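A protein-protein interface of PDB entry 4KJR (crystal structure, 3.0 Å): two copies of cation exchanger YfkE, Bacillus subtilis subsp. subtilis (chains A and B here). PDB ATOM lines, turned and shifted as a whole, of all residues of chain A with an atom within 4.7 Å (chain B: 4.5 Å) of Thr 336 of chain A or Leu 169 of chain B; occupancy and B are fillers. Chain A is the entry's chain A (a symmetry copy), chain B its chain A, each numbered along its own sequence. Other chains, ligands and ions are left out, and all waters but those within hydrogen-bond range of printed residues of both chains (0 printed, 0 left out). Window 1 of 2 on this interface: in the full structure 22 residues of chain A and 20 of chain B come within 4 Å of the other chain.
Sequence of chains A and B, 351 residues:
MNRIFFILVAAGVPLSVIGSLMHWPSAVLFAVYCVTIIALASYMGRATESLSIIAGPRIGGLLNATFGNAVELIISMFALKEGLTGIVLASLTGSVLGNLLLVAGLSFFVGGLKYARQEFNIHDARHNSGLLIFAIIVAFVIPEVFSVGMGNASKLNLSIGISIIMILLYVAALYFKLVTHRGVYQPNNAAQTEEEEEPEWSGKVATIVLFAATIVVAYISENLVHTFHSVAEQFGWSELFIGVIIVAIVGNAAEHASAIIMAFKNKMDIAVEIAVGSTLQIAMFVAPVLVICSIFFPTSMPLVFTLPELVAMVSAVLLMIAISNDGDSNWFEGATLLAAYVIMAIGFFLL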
ATOM      1  N   PHE A 332      26.848   8.845 -29.492  1.00  0.00           N
ATOM      2  CA  PHE A 332      27.345   9.392 -28.235  1.00  0.00           C
ATOM      3  C   PHE A 332      27.282   8.377 -27.091  1.00  0.00           C
ATOM      4  O   PHE A 332      27.477   8.723 -25.926  1.00  0.00           O
ATOM      5  CB  PHE A 332      26.623  10.702 -27.889  1.00  0.00           C
ATOM      6  CG  PHE A 332      25.397  10.528 -27.038  1.00  0.00           C
ATOM      7  CD1 PHE A 332      25.327  11.121 -25.781  1.00  0.00           C
ATOM      8  CD2 PHE A 332      24.315   9.780 -27.487  1.00  0.00           C
ATOM      9  CE1 PHE A 332      24.203  10.972 -24.986  1.00  0.00           C
ATOM     10  CE2 PHE A 332      23.189   9.624 -26.694  1.00  0.00           C
ATOM     11  CZ  PHE A 332      23.132  10.223 -25.443  1.00  0.00           C
ATOM     12  N   GLU A 333      27.019   7.117 -27.436  1.00  0.00           N
ATOM     13  CA  GLU A 333      27.190   6.012 -26.501  1.00  0.00           C
ATOM     14  C   GLU A 333      28.628   6.047 -26.005  1.00  0.00           C
ATOM     15  O   GLU A 333      28.897   5.809 -24.829  1.00  0.00           O
ATOM     16  CB  GLU A 333      26.940   4.685 -27.210  1.00  0.00           C
ATOM     17  CG  GLU A 333      26.232   3.629 -26.377  1.00  0.00           C
ATOM     18  CD  GLU A 333      24.726   3.801 -26.373  1.00  0.00           C
ATOM     19  OE1 GLU A 333      24.237   4.751 -25.727  1.00  0.00           O
ATOM     20  OE2 GLU A 333      24.029   2.983 -27.009  1.00  0.00           O
ATOM     21  N   GLY A 334      29.541   6.356 -26.923  1.00  0.00           N
ATOM     22  CA  GLY A 334      30.958   6.465 -26.620  1.00  0.00           C
ATOM     23  C   GLY A 334      31.298   7.780 -25.960  1.00  0.00           C
ATOM     24  O   GLY A 334      32.098   7.818 -25.017  1.00  0.00           O
ATOM     25  N   ALA A 335      30.693   8.860 -26.459  1.00  0.00           N
ATOM     26  CA  ALA A 335      30.948  10.205 -25.939  1.00  0.00           C
ATOM     27  C   ALA A 335      30.686  10.275 -24.442  1.00  0.00           C
ATOM     28  O   ALA A 335      31.489  10.834 -23.690  1.00  0.00           O
ATOM     29  CB  ALA A 335      30.113  11.241 -26.678  1.00  0.00           C
ATOM     30  N   THR A 336      29.568   9.689 -24.021  1.00  0.00           N
ATOM     31  CA  THR A 336      29.233   9.581 -22.609  1.00  0.00           C
ATOM     32  C   THR A 336      30.386   8.889 -21.891  1.00  0.00           C
ATOM     33  O   THR A 336      30.910   9.405 -20.903  1.00  0.00           O
ATOM     34  CB  THR A 336      27.933   8.786 -22.387  1.00  0.00           C
ATOM     35  OG1 THR A 336      27.225   8.653 -23.624  1.00  0.00           O
ATOM     36  CG2 THR A 336      27.045   9.495 -21.389  1.00  0.00           C
ATOM     37  N   LEU A 337      30.811   7.747 -22.425  1.00  0.00           N
ATOM     38  CA  LEU A 337      31.896   6.970 -21.825  1.00  0.00           C
ATOM     39  C   LEU A 337      33.197   7.756 -21.766  1.00  0.00           C
ATOM     40  O   LEU A 337      33.749   7.939 -20.687  1.00  0.00           O
ATOM     41  CB  LEU A 337      32.106   5.638 -22.555  1.00  0.00           C
ATOM     42  CG  LEU A 337      31.037   4.542 -22.482  1.00  0.00           C
ATOM     43  CD1 LEU A 337      31.506   3.317 -23.254  1.00  0.00           C
ATOM     44  CD2 LEU A 337      30.696   4.160 -21.050  1.00  0.00           C
ATOM     45  N   LEU A 338      33.661   8.246 -22.914  1.00  0.00           N
ATOM     46  CA  LEU A 338      34.938   8.968 -23.002  1.00  0.00           C
ATOM     47  C   LEU A 338      35.013  10.132 -22.023  1.00  0.00           C
ATOM     48  O   LEU A 338      36.061  10.390 -21.412  1.00  0.00           O
ATOM     49  CB  LEU A 338      35.169   9.464 -24.427  1.00  0.00           C
ATOM     50  CG  LEU A 338      35.537   8.373 -25.435  1.00  0.00           C
ATOM     51  CD1 LEU A 338      35.101   8.785 -26.826  1.00  0.00           C
ATOM     52  CD2 LEU A 338      37.026   8.052 -25.406  1.00  0.00           C
ATOM     53  N   ALA A 339      33.879  10.820 -21.883  1.00  0.00           N
ATOM     54  CA  ALA A 339      33.713  11.897 -20.924  1.00  0.00           C
ATOM     55  C   ALA A 339      33.985  11.373 -19.522  1.00  0.00           C
ATOM     56  O   ALA A 339      34.831  11.915 -18.808  1.00  0.00           O
ATOM     57  CB  ALA A 339      32.308  12.468 -21.019  1.00  0.00           C
ATOM     58  N   ALA A 340      33.289  10.303 -19.144  1.00  0.00           N
ATOM     59  CA  ALA A 340      33.435   9.741 -17.804  1.00  0.00           C
ATOM     60  C   ALA A 340      34.887   9.399 -17.521  1.00  0.00           C
ATOM     61  O   ALA A 340      35.415   9.751 -16.463  1.00  0.00           O
ATOM     62  CB  ALA A 340      32.545   8.525 -17.622  1.00  0.00           C
ATOM     63  N   PHE B 134      25.416   7.222 -15.590  1.00  0.00           N
ATOM     64  CA  PHE B 134      26.521   8.088 -15.983  1.00  0.00           C
ATOM     65  C   PHE B 134      26.471   9.461 -15.315  1.00  0.00           C
ATOM     66  O   PHE B 134      27.450   9.903 -14.742  1.00  0.00           O
ATOM     67  CB  PHE B 134      26.584   8.294 -17.501  1.00  0.00           C
ATOM     68  CG  PHE B 134      27.205   9.608 -17.885  1.00  0.00           C
ATOM     69  CD1 PHE B 134      28.513   9.682 -18.367  1.00  0.00           C
ATOM     70  CD2 PHE B 134      26.496  10.788 -17.704  1.00  0.00           C
ATOM     71  CE1 PHE B 134      29.083  10.907 -18.683  1.00  0.00           C
ATOM     72  CE2 PHE B 134      27.057  12.012 -18.009  1.00  0.00           C
ATOM     73  CZ  PHE B 134      28.353  12.073 -18.510  1.00  0.00           C
ATOM     74  N   ILE B 165      32.127  19.675 -19.152  1.00  0.00           N
ATOM     75  CA  ILE B 165      31.884  18.526 -20.027  1.00  0.00           C
ATOM     76  C   ILE B 165      30.434  18.048 -19.973  1.00  0.00           C
ATOM     77  O   ILE B 165      29.934  17.494 -20.948  1.00  0.00           O
ATOM     78  CB  ILE B 165      32.841  17.335 -19.771  1.00  0.00           C
ATOM     79  CG1 ILE B 165      32.465  16.583 -18.491  1.00  0.00           C
ATOM     80  CG2 ILE B 165      34.296  17.783 -19.777  1.00  0.00           C
ATOM     81  CD1 ILE B 165      31.545  15.395 -18.711  1.00  0.00           C
ATOM     82  N   MET B 166      29.768  18.258 -18.838  1.00  0.00           N
ATOM     83  CA  MET B 166      28.382  17.824 -18.662  1.00  0.00           C
ATOM     84  C   MET B 166      27.463  18.631 -19.542  1.00  0.00           C
ATOM     85  O   MET B 166      26.636  18.062 -20.252  1.00  0.00           O
ATOM     86  CB  MET B 166      27.973  17.913 -17.197  1.00  0.00           C
ATOM     87  CG  MET B 166      28.340  16.629 -16.460  1.00  0.00           C
ATOM     88  SD  MET B 166      27.510  16.633 -14.668  1.00  0.00           S
ATOM     89  CE  MET B 166      28.563  18.058 -13.815  1.00  0.00           C
ATOM     90  N   ILE B 167      27.603  19.958 -19.510  1.00  0.00           N
ATOM     91  CA  ILE B 167      26.864  20.844 -20.412  1.00  0.00           C
ATOM     92  C   ILE B 167      27.281  20.611 -21.862  1.00  0.00           C
ATOM     93  O   ILE B 167      26.434  20.355 -22.720  1.00  0.00           O
ATOM     94  CB  ILE B 167      27.052  22.331 -20.035  1.00  0.00           C
ATOM     95  CG1 ILE B 167      26.127  22.708 -18.885  1.00  0.00           C
ATOM     96  CG2 ILE B 167      26.771  23.254 -21.209  1.00  0.00           C
ATOM     97  CD1 ILE B 167      26.821  22.763 -17.547  1.00  0.00           C
ATOM     98  N   LEU B 168      28.589  20.678 -22.122  1.00  0.00           N
ATOM     99  CA  LEU B 168      29.126  20.489 -23.470  1.00  0.00           C
ATOM    100  C   LEU B 168      28.662  19.161 -24.077  1.00  0.00           C
ATOM    101  O   LEU B 168      28.534  19.050 -25.291  1.00  0.00           O
ATOM    102  CB  LEU B 168      30.655  20.549 -23.450  1.00  0.00           C
ATOM    103  CG  LEU B 168      31.274  21.894 -23.057  1.00  0.00           C
ATOM    104  CD1 LEU B 168      32.785  21.772 -22.934  1.00  0.00           C
ATOM    105  CD2 LEU B 168      30.898  22.974 -24.060  1.00  0.00           C
ATOM    106  N   LEU B 169      28.394  18.165 -23.233  1.00  0.00           N
ATOM    107  CA  LEU B 169      27.824  16.918 -23.720  1.00  0.00           C
ATOM    108  C   LEU B 169      26.320  17.062 -23.837  1.00  0.00           C
ATOM    109  O   LEU B 169      25.735  16.671 -24.846  1.00  0.00           O
ATOM    110  CB  LEU B 169      28.173  15.725 -22.821  1.00  0.00           C
ATOM    111  CG  LEU B 169      28.197  14.369 -23.544  1.00  0.00           C
ATOM    112  CD1 LEU B 169      29.561  14.159 -24.192  1.00  0.00           C
ATOM    113  CD2 LEU B 169      27.856  13.200 -22.625  1.00  0.00           C
ATOM    114  N   TYR B 170      25.704  17.632 -22.804  1.00  0.00           N
ATOM    115  CA  TYR B 170      24.254  17.782 -22.760  1.00  0.00           C
ATOM    116  C   TYR B 170      23.742  18.626 -23.917  1.00  0.00           C
ATOM    117  O   TYR B 170      22.763  18.265 -24.566  1.00  0.00           O
ATOM    118  CB  TYR B 170      23.794  18.379 -21.431  1.00  0.00           C
ATOM    119  CG  TYR B 170      22.295  18.449 -21.305  1.00  0.00           C
ATOM    120  CD1 TYR B 170      21.536  17.288 -21.181  1.00  0.00           C
ATOM    121  CD2 TYR B 170      21.635  19.670 -21.325  1.00  0.00           C
ATOM    122  CE1 TYR B 170      20.157  17.342 -21.067  1.00  0.00           C
ATOM    123  CE2 TYR B 170      20.255  19.737 -21.209  1.00  0.00           C
ATOM    124  CZ  TYR B 170      19.521  18.572 -21.080  1.00  0.00           C
ATOM    125  OH  TYR B 170      18.150  18.633 -20.972  1.00  0.00           O
ATOM    126  N   VAL B 171      24.411  19.745 -24.175  1.00  0.00           N
ATOM    127  CA  VAL B 171      24.071  20.576 -25.322  1.00  0.00           C
ATOM    128  C   VAL B 171      24.364  19.808 -26.611  1.00  0.00           C
ATOM    129  O   VAL B 171      23.558  19.827 -27.543  1.00  0.00           O
ATOM    130  CB  VAL B 171      24.795  21.942 -25.293  1.00  0.00           C
ATOM    131  CG1 VAL B 171      24.371  22.805 -26.473  1.00  0.00           C
ATOM    132  CG2 VAL B 171      24.484  22.673 -23.997  1.00  0.00           C
ATOM    133  N   ALA B 172      25.498  19.105 -26.643  1.00  0.00           N
ATOM    134  CA  ALA B 172      25.890  18.311 -27.810  1.00  0.00           C
ATOM    135  C   ALA B 172      24.881  17.210 -28.117  1.00  0.00           C
ATOM    136  O   ALA B 172      24.536  16.994 -29.277  1.00  0.00           O
ATOM    137  CB  ALA B 172      27.280  17.724 -27.630  1.00  0.00           C
ATOM    138  N   ALA B 173      24.407  16.530 -27.075  1.00  0.00           N
ATOM    139  CA  ALA B 173      23.413  15.475 -27.232  1.00  0.00           C
ATOM    140  C   ALA B 173      22.038  16.055 -27.548  1.00  0.00           C
ATOM    141  O   ALA B 173      21.457  15.719 -28.574  1.00  0.00           O
ATOM    142  CB  ALA B 173      23.357  14.596 -25.992  1.00  0.00           C
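Ala 173 of chain B touches Phe 332 of chain A (CB to CE1, 3.9 Å).
Leu 169 of chain B touches Ala 335 of chain A.
Thr 336 of chain A touches Phe 134 of chain B.
CA of Thr 336 of chain A touches CD2 of Leu 169 of chain B, at 3.9 Å.
Ala 339 of chain A touches Ile 165 of chain B (CB to CD1, 3.8 Å).
Of the printed residues of chain B, Thr 336 of chain A touches Phe 134 and Leu 169.
Leu 337 of chain A touches none of the printed residues of chain B.
Printed residues of chain B within 4 Å of Ala 339 of chain A: Ile 165 (3.8 Å).
Of the printed residues of chain A, Phe 134 of chain B touches Thr 336.
Ile 167 of chain B touches none of the printed residues of chain A.
The nearest printed residue of chain A that does not touch Phe 134 of chain B is Ala 340 of chain A (4.3 Å).
Hydrophobic or aromatic side chains of chain A that line the printed part of chain B: Phe 332, Ala 335 and Ala 339.
Hydrophobic or aromatic side chains of chain B that line the printed part of chain A: Phe 134, Ile 165, Leu 169 and Ala 173.
Among the printed residues, 5 pairs touch across the chains.
Among the printed residues, no Asp or Glu carboxylate lies within 4 Å of a Lys or Arg side-chain nitrogen of the other chain.
No position is printed for both chains.
Of the 5 pairs that touch across the chains among the printed residues, none has its exchanged pair printed and touching as well.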
